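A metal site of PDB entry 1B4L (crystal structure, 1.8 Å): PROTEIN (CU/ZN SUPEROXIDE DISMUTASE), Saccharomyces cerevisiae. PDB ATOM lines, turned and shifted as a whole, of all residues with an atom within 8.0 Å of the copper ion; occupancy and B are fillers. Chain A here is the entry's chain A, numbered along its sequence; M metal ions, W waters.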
ATOM      1  N   GLY A  44      19.584   4.315 -11.309  1.00  0.00           N
ATOM      2  CA  GLY A  44      19.839   3.842  -9.963  1.00  0.00           C
ATOM      3  C   GLY A  44      20.952   4.634  -9.288  1.00  0.00           C
ATOM      4  O   GLY A  44      22.037   4.786  -9.835  1.00  0.00           O
ATOM      5  N   PHE A  45      20.688   5.032  -8.044  1.00  0.00           N
ATOM      6  CA  PHE A  45      21.581   5.872  -7.244  1.00  0.00           C
ATOM      7  C   PHE A  45      21.750   5.182  -5.904  1.00  0.00           C
ATOM      8  O   PHE A  45      20.787   5.069  -5.155  1.00  0.00           O
ATOM      9  CB  PHE A  45      20.874   7.218  -7.035  1.00  0.00           C
ATOM     10  CG  PHE A  45      21.781   8.347  -6.629  1.00  0.00           C
ATOM     11  CD1 PHE A  45      23.093   8.431  -7.084  1.00  0.00           C
ATOM     12  CD2 PHE A  45      21.294   9.365  -5.826  1.00  0.00           C
ATOM     13  CE1 PHE A  45      23.892   9.504  -6.757  1.00  0.00           C
ATOM     14  CE2 PHE A  45      22.093  10.456  -5.487  1.00  0.00           C
ATOM     15  CZ  PHE A  45      23.396  10.518  -5.958  1.00  0.00           C
ATOM     16  N   HIS A  46      22.947   4.732  -5.576  1.00  0.00           N
ATOM     17  CA  HIS A  46      23.136   4.023  -4.310  1.00  0.00           C
ATOM     18  C   HIS A  46      24.440   4.300  -3.621  1.00  0.00           C
ATOM     19  O   HIS A  46      25.415   4.645  -4.256  1.00  0.00           O
ATOM     20  CB  HIS A  46      23.116   2.507  -4.534  1.00  0.00           C
ATOM     21  CG  HIS A  46      22.035   2.024  -5.433  1.00  0.00           C
ATOM     22  ND1 HIS A  46      22.289   1.303  -6.572  1.00  0.00           N
ATOM     23  CD2 HIS A  46      20.695   2.217  -5.395  1.00  0.00           C
ATOM     24  CE1 HIS A  46      21.139   1.077  -7.209  1.00  0.00           C
ATOM     25  NE2 HIS A  46      20.172   1.626  -6.513  1.00  0.00           N
ATOM     26  N   ILE A  47      24.454   4.007  -2.326  1.00  0.00           N
ATOM     27  CA  ILE A  47      25.668   4.113  -1.552  1.00  0.00           C
ATOM     28  C   ILE A  47      26.142   2.669  -1.433  1.00  0.00           C
ATOM     29  O   ILE A  47      25.368   1.787  -1.067  1.00  0.00           O
ATOM     30  CB  ILE A  47      25.429   4.712  -0.156  1.00  0.00           C
ATOM     31  CG1 ILE A  47      25.054   6.189  -0.310  1.00  0.00           C
ATOM     32  CG2 ILE A  47      26.682   4.547   0.712  1.00  0.00           C
ATOM     33  CD1 ILE A  47      24.663   6.877   0.948  1.00  0.00           C
ATOM     34  N   HIS A  48      27.350   2.403  -1.914  1.00  0.00           N
ATOM     35  CA  HIS A  48      27.918   1.071  -1.813  1.00  0.00           C
ATOM     36  C   HIS A  48      28.832   1.004  -0.582  1.00  0.00           C
ATOM     37  O   HIS A  48      29.321   2.041  -0.093  1.00  0.00           O
ATOM     38  CB  HIS A  48      28.661   0.691  -3.092  1.00  0.00           C
ATOM     39  CG  HIS A  48      27.739   0.429  -4.247  1.00  0.00           C
ATOM     40  ND1 HIS A  48      27.836  -0.708  -5.021  1.00  0.00           N
ATOM     41  CD2 HIS A  48      26.692   1.128  -4.739  1.00  0.00           C
ATOM     42  CE1 HIS A  48      26.882  -0.700  -5.941  1.00  0.00           C
ATOM     43  NE2 HIS A  48      26.178   0.411  -5.785  1.00  0.00           N
ATOM     44  N   GLY A  61      32.106  -2.528  -4.017  1.00  0.00           N
ATOM     45  CA  GLY A  61      31.323  -3.605  -3.433  1.00  0.00           C
ATOM     46  C   GLY A  61      29.829  -3.515  -3.629  1.00  0.00           C
ATOM     47  O   GLY A  61      29.371  -2.854  -4.558  1.00  0.00           O
ATOM     48  N   PRO A  62      29.042  -4.184  -2.762  1.00  0.00           N
ATOM     49  CA  PRO A  62      27.568  -4.221  -2.815  1.00  0.00           C
ATOM     50  C   PRO A  62      26.935  -3.002  -2.144  1.00  0.00           C
ATOM     51  O   PRO A  62      27.645  -2.123  -1.637  1.00  0.00           O
ATOM     52  CB  PRO A  62      27.253  -5.491  -2.024  1.00  0.00           C
ATOM     53  CG  PRO A  62      28.264  -5.445  -0.931  1.00  0.00           C
ATOM     54  CD  PRO A  62      29.546  -5.013  -1.645  1.00  0.00           C
ATOM     55  N   HIS A  63      25.615  -2.929  -2.152  1.00  0.00           N
ATOM     56  CA  HIS A  63      24.927  -1.810  -1.528  1.00  0.00           C
ATOM     57  C   HIS A  63      25.214  -1.869  -0.016  1.00  0.00           C
ATOM     58  O   HIS A  63      25.349  -2.957   0.548  1.00  0.00           O
ATOM     59  CB  HIS A  63      23.419  -1.896  -1.762  1.00  0.00           C
ATOM     60  CG  HIS A  63      23.016  -1.704  -3.197  1.00  0.00           C
ATOM     61  ND1 HIS A  63      21.720  -1.845  -3.633  1.00  0.00           N
ATOM     62  CD2 HIS A  63      23.746  -1.348  -4.282  1.00  0.00           C
ATOM     63  CE1 HIS A  63      21.666  -1.590  -4.931  1.00  0.00           C
ATOM     64  NE2 HIS A  63      22.880  -1.283  -5.343  1.00  0.00           N
ATOM     65  N   PHE A  64      25.372  -0.707   0.600  1.00  0.00           N
ATOM     66  CA  PHE A  64      25.634  -0.618   2.031  1.00  0.00           C
ATOM     67  C   PHE A  64      24.373  -1.188   2.687  1.00  0.00           C
ATOM     68  O   PHE A  64      23.307  -0.598   2.581  1.00  0.00           O
ATOM     69  CB  PHE A  64      25.876   0.839   2.452  1.00  0.00           C
ATOM     70  CG  PHE A  64      26.279   1.010   3.896  1.00  0.00           C
ATOM     71  CD1 PHE A  64      27.140   0.093   4.513  1.00  0.00           C
ATOM     72  CD2 PHE A  64      25.811   2.076   4.647  1.00  0.00           C
ATOM     73  CE1 PHE A  64      27.503   0.236   5.839  1.00  0.00           C
ATOM     74  CE2 PHE A  64      26.178   2.230   5.981  1.00  0.00           C
ATOM     75  CZ  PHE A  64      27.022   1.317   6.575  1.00  0.00           C
ATOM     76  N   HIS A  71      16.996  -5.450  -1.157  1.00  0.00           N
ATOM     77  CA  HIS A  71      16.946  -4.191  -1.892  1.00  0.00           C
ATOM     78  C   HIS A  71      15.531  -3.684  -2.004  1.00  0.00           C
ATOM     79  O   HIS A  71      14.614  -4.466  -2.205  1.00  0.00           O
ATOM     80  CB  HIS A  71      17.565  -4.381  -3.286  1.00  0.00           C
ATOM     81  CG  HIS A  71      17.563  -3.137  -4.116  1.00  0.00           C
ATOM     82  ND1 HIS A  71      18.526  -2.148  -3.976  1.00  0.00           N
ATOM     83  CD2 HIS A  71      16.686  -2.689  -5.045  1.00  0.00           C
ATOM     84  CE1 HIS A  71      18.221  -1.141  -4.783  1.00  0.00           C
ATOM     85  NE2 HIS A  71      17.113  -1.450  -5.440  1.00  0.00           N
ATOM     86  N   HIS A  80      17.927  -1.426   1.585  1.00  0.00           N
ATOM     87  CA  HIS A  80      19.307  -1.354   2.061  1.00  0.00           C
ATOM     88  C   HIS A  80      19.499   0.112   2.523  1.00  0.00           C
ATOM     89  O   HIS A  80      18.846   1.007   1.994  1.00  0.00           O
ATOM     90  CB  HIS A  80      20.282  -1.594   0.897  1.00  0.00           C
ATOM     91  CG  HIS A  80      20.201  -2.966   0.321  1.00  0.00           C
ATOM     92  ND1 HIS A  80      20.506  -3.246  -0.998  1.00  0.00           N
ATOM     93  CD2 HIS A  80      19.929  -4.157   0.912  1.00  0.00           C
ATOM     94  CE1 HIS A  80      20.430  -4.550  -1.186  1.00  0.00           C
ATOM     95  NE2 HIS A  80      20.080  -5.122  -0.046  1.00  0.00           N
ATOM     96  N   GLY A  82      21.893   2.022   1.853  1.00  0.00           N
ATOM     97  CA  GLY A  82      22.386   2.735   0.681  1.00  0.00           C
ATOM     98  C   GLY A  82      21.433   2.928  -0.488  1.00  0.00           C
ATOM     99  O   GLY A  82      21.819   3.512  -1.510  1.00  0.00           O
ATOM    100  N   ASP A  83      20.193   2.459  -0.347  1.00  0.00           N
ATOM    101  CA  ASP A  83      19.183   2.557  -1.389  1.00  0.00           C
ATOM    102  C   ASP A  83      18.567   3.948  -1.524  1.00  0.00           C
ATOM    103  O   ASP A  83      17.723   4.372  -0.729  1.00  0.00           O
ATOM    104  CB  ASP A  83      18.081   1.505  -1.186  1.00  0.00           C
ATOM    105  CG  ASP A  83      18.560   0.090  -1.510  1.00  0.00           C
ATOM    106  OD1 ASP A  83      19.655  -0.101  -2.088  1.00  0.00           O
ATOM    107  OD2 ASP A  83      17.860  -0.883  -1.181  1.00  0.00           O
ATOM    108  N   MET A  84      19.015   4.659  -2.553  1.00  0.00           N
ATOM    109  CA  MET A  84      18.511   5.999  -2.830  1.00  0.00           C
ATOM    110  C   MET A  84      17.579   6.024  -4.054  1.00  0.00           C
ATOM    111  O   MET A  84      17.196   7.090  -4.518  1.00  0.00           O
ATOM    112  CB  MET A  84      19.665   7.009  -2.963  1.00  0.00           C
ATOM    113  CG  MET A  84      20.583   7.047  -1.743  1.00  0.00           C
ATOM    114  SD  MET A  84      21.826   8.323  -1.800  1.00  0.00           S
ATOM    115  CE  MET A  84      23.022   7.544  -2.869  1.00  0.00           C
ATOM    116  N   GLY A  85      17.212   4.841  -4.555  1.00  0.00           N
ATOM    117  CA  GLY A  85      16.291   4.753  -5.664  1.00  0.00           C
ATOM    118  C   GLY A  85      16.824   5.135  -7.016  1.00  0.00           C
ATOM    119  O   GLY A  85      17.910   4.683  -7.398  1.00  0.00           O
ATOM    120  N   SER A 116      31.134   4.617  -0.681  1.00  0.00           N
ATOM    121  CA  SER A 116      31.009   5.115  -2.043  1.00  0.00           C
ATOM    122  C   SER A 116      29.597   5.434  -2.480  1.00  0.00           C
ATOM    123  O   SER A 116      28.647   4.851  -1.996  1.00  0.00           O
ATOM    124  CB  SER A 116      31.565   4.081  -3.038  1.00  0.00           C
ATOM    125  OG  SER A 116      32.980   4.124  -3.092  1.00  0.00           O
ATOM    126  N   VAL A 117      29.508   6.363  -3.432  1.00  0.00           N
ATOM    127  CA  VAL A 117      28.240   6.747  -4.051  1.00  0.00           C
ATOM    128  C   VAL A 117      28.439   6.288  -5.509  1.00  0.00           C
ATOM    129  O   VAL A 117      29.472   6.589  -6.125  1.00  0.00           O
ATOM    130  CB  VAL A 117      28.009   8.274  -4.082  1.00  0.00           C
ATOM    131  CG1 VAL A 117      26.790   8.573  -4.953  1.00  0.00           C
ATOM    132  CG2 VAL A 117      27.775   8.811  -2.692  1.00  0.00           C
ATOM    133  N   VAL A 118      27.465   5.536  -6.031  1.00  0.00           N
ATOM    134  CA  VAL A 118      27.514   5.011  -7.392  1.00  0.00           C
ATOM    135  C   VAL A 118      26.238   5.370  -8.163  1.00  0.00           C
ATOM    136  O   VAL A 118      25.130   5.235  -7.641  1.00  0.00           O
ATOM    137  CB  VAL A 118      27.648   3.443  -7.393  1.00  0.00           C
ATOM    138  CG1 VAL A 118      27.565   2.879  -8.821  1.00  0.00           C
ATOM    139  CG2 VAL A 118      28.964   3.030  -6.744  1.00  0.00           C
ATOM    140  N   ILE A 119      26.408   5.843  -9.389  1.00  0.00           N
ATOM    141  CA  ILE A 119      25.288   6.152 -10.263  1.00  0.00           C
ATOM    142  C   ILE A 119      25.340   5.026 -11.298  1.00  0.00           C
ATOM    143  O   ILE A 119      26.424   4.661 -11.790  1.00  0.00           O
ATOM    144  CB  ILE A 119      25.441   7.563 -10.948  1.00  0.00           C
ATOM    145  CG1 ILE A 119      24.193   7.913 -11.761  1.00  0.00           C
ATOM    146  CG2 ILE A 119      26.691   7.616 -11.840  1.00  0.00           C
ATOM    147  CD1 ILE A 119      22.923   7.940 -10.947  1.00  0.00           C
ATOM    148  N   HIS A 120      24.204   4.407 -11.563  1.00  0.00           N
ATOM    149  CA  HIS A 120      24.165   3.307 -12.522  1.00  0.00           C
ATOM    150  C   HIS A 120      23.755   3.716 -13.940  1.00  0.00           C
ATOM    151  O   HIS A 120      23.269   4.839 -14.161  1.00  0.00           O
ATOM    152  CB  HIS A 120      23.227   2.202 -12.022  1.00  0.00           C
ATOM    153  CG  HIS A 120      23.749   1.501 -10.815  1.00  0.00           C
ATOM    154  ND1 HIS A 120      24.518   0.369 -10.898  1.00  0.00           N
ATOM    155  CD2 HIS A 120      23.650   1.806  -9.498  1.00  0.00           C
ATOM    156  CE1 HIS A 120      24.885   0.002  -9.683  1.00  0.00           C
ATOM    157  NE2 HIS A 120      24.379   0.853  -8.813  1.00  0.00           N
ATOM    158  N   ASP A 124      16.712   1.429 -11.671  1.00  0.00           N
ATOM    159  CA  ASP A 124      16.578   0.605 -10.481  1.00  0.00           C
ATOM    160  C   ASP A 124      15.135   0.085 -10.417  1.00  0.00           C
ATOM    161  O   ASP A 124      14.199   0.891 -10.333  1.00  0.00           O
ATOM    162  CB  ASP A 124      16.888   1.481  -9.256  1.00  0.00           C
ATOM    163  CG  ASP A 124      16.920   0.713  -7.950  1.00  0.00           C
ATOM    164  OD1 ASP A 124      16.341  -0.393  -7.856  1.00  0.00           O
ATOM    165  OD2 ASP A 124      17.534   1.252  -7.012  1.00  0.00           O
ATOM    166  N   LYS A 136      18.798  -7.847  -4.757  1.00  0.00           N
ATOM    167  CA  LYS A 136      20.169  -7.541  -4.351  1.00  0.00           C
ATOM    168  C   LYS A 136      20.621  -6.173  -4.851  1.00  0.00           C
ATOM    169  O   LYS A 136      21.054  -5.323  -4.079  1.00  0.00           O
ATOM    170  CB  LYS A 136      21.149  -8.590  -4.882  1.00  0.00           C
ATOM    171  CG  LYS A 136      20.881  -9.987  -4.385  1.00  0.00           C
ATOM    172  CD  LYS A 136      22.003 -10.933  -4.792  1.00  0.00           C
ATOM    173  CE  LYS A 136      21.449 -12.292  -5.251  1.00  0.00           C
ATOM    174  NZ  LYS A 136      20.867 -12.237  -6.653  1.00  0.00           N
ATOM    175  N   THR A 137      20.410  -5.955  -6.141  1.00  0.00           N
ATOM    176  CA  THR A 137      20.838  -4.735  -6.830  1.00  0.00           C
ATOM    177  C   THR A 137      19.716  -3.943  -7.491  1.00  0.00           C
ATOM    178  O   THR A 137      19.923  -2.777  -7.845  1.00  0.00           O
ATOM    179  CB  THR A 137      21.818  -5.103  -7.984  1.00  0.00           C
ATOM    180  OG1 THR A 137      21.094  -5.730  -9.059  1.00  0.00           O
ATOM    181  CG2 THR A 137      22.911  -6.053  -7.482  1.00  0.00           C
ATOM    182  N   GLY A 138      18.547  -4.552  -7.701  1.00  0.00           N
ATOM    183  CA  GLY A 138      17.466  -3.854  -8.365  1.00  0.00           C
ATOM    184  C   GLY A 138      17.680  -3.829  -9.875  1.00  0.00           C
ATOM    185  O   GLY A 138      17.038  -3.042 -10.576  1.00  0.00           O
ATOM    186  N   ALA A 140      19.951  -2.607 -11.646  1.00  0.00           N
ATOM    187  CA  ALA A 140      20.356  -1.274 -12.099  1.00  0.00           C
ATOM    188  C   ALA A 140      21.465  -1.261 -13.168  1.00  0.00           C
ATOM    189  O   ALA A 140      21.704  -0.229 -13.798  1.00  0.00           O
ATOM    190  CB  ALA A 140      20.735  -0.411 -10.893  1.00  0.00           C
ATOM    191  N   GLY A 141      22.169  -2.377 -13.315  1.00  0.00           N
ATOM    192  CA  GLY A 141      23.222  -2.479 -14.308  1.00  0.00           C
ATOM    193  C   GLY A 141      24.625  -1.951 -13.977  1.00  0.00           C
ATOM    194  O   GLY A 141      25.024  -1.863 -12.798  1.00  0.00           O
ATOM    195  N   PRO A 142      25.407  -1.620 -15.017  1.00  0.00           N
ATOM    196  CA  PRO A 142      26.787  -1.103 -14.915  1.00  0.00           C
ATOM    197  C   PRO A 142      26.895   0.179 -14.059  1.00  0.00           C
ATOM    198  O   PRO A 142      25.902   0.872 -13.824  1.00  0.00           O
ATOM    199  CB  PRO A 142      27.168  -0.869 -16.374  1.00  0.00           C
ATOM    200  CG  PRO A 142      26.275  -1.845 -17.135  1.00  0.00           C
ATOM    201  CD  PRO A 142      24.984  -1.719 -16.425  1.00  0.00           C
ATOM    202  N   ARG A 143      28.123   0.469 -13.644  1.00  0.00           N
ATOM    203  CA  ARG A 143      28.417   1.608 -12.785  1.00  0.00           C
ATOM    204  C   ARG A 143      29.363   2.555 -13.527  1.00  0.00           C
ATOM    205  O   ARG A 143      30.579   2.484 -13.338  1.00  0.00           O
ATOM    206  CB  ARG A 143      29.127   1.111 -11.516  1.00  0.00           C
ATOM    207  CG  ARG A 143      28.499  -0.099 -10.851  1.00  0.00           C
ATOM    208  CD  ARG A 143      29.323  -0.569  -9.657  1.00  0.00           C
ATOM    209  NE  ARG A 143      28.759  -1.779  -9.051  1.00  0.00           N
ATOM    210  CZ  ARG A 143      29.198  -2.347  -7.936  1.00  0.00           C
ATOM    211  NH1 ARG A 143      30.219  -1.848  -7.259  1.00  0.00           N
ATOM    212  NH2 ARG A 143      28.598  -3.439  -7.479  1.00  0.00           N
HETATM  213 CU    CU M   1      24.197   0.587  -6.836  1.00  0.00          CU
HETATM  214 ZN    ZN M   2      20.115  -1.878  -2.542  1.00  0.00          ZN
HETATM  215  O   HOH W   1      24.821  -2.432  -7.745  1.00  0.00           O
HETATM  216  O   HOH W   2      22.292  -1.601  -8.099  1.00  0.00           O
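Water W2 lies within hydrogen-bond range of the backbone carbonyl oxygen (O) of Thr 137 and a ring nitrogen (NE2) of His 63.
The copper ion is bound by NE2 of His 120 (2.0 Å), ND1 of His 46 (2.1 Å) and NE2 of His 48 (2.2 Å).
Slightly farther from the copper ion lies a ring nitrogen (NE2) of His 63 (2.7 Å).
O of His 46 is in hydrogen-bond range of N of Val 118 (2.9 Å).
A ring nitrogen (ND1) of His 48 is in hydrogen-bond range of the backbone carbonyl oxygen (O) of Gly 61 (2.7 Å).
A ring nitrogen (ND1) of His 120 sits at hydrogen-bond distance from the backbone carbonyl oxygen of Gly 141 (3.0 Å).
N of His 48 lies within hydrogen-bond range of O of Ser 116, at 2.8 Å.
A ring nitrogen (NE2) of His 46 sits at hydrogen-bond distance from the side-chain carboxylate of Asp 124 (2.7 Å).
The backbone NH (N) of His 120 sits at hydrogen-bond distance from the backbone carbonyl oxygen (O) of Gly 44, 2.8 Å away.
A ring nitrogen (ND1) of His 48 lies within hydrogen-bond range of the guanidinium group of Arg 143 (3.5 Å).
The backbone carbonyl oxygen (O) of Pro 142 lies close to a ring nitrogen (ND1) of His 120 (3.3 Å).
Four residues have an atom within 4 Å of the copper ion: His 46, His 48, His 63 and His 120.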
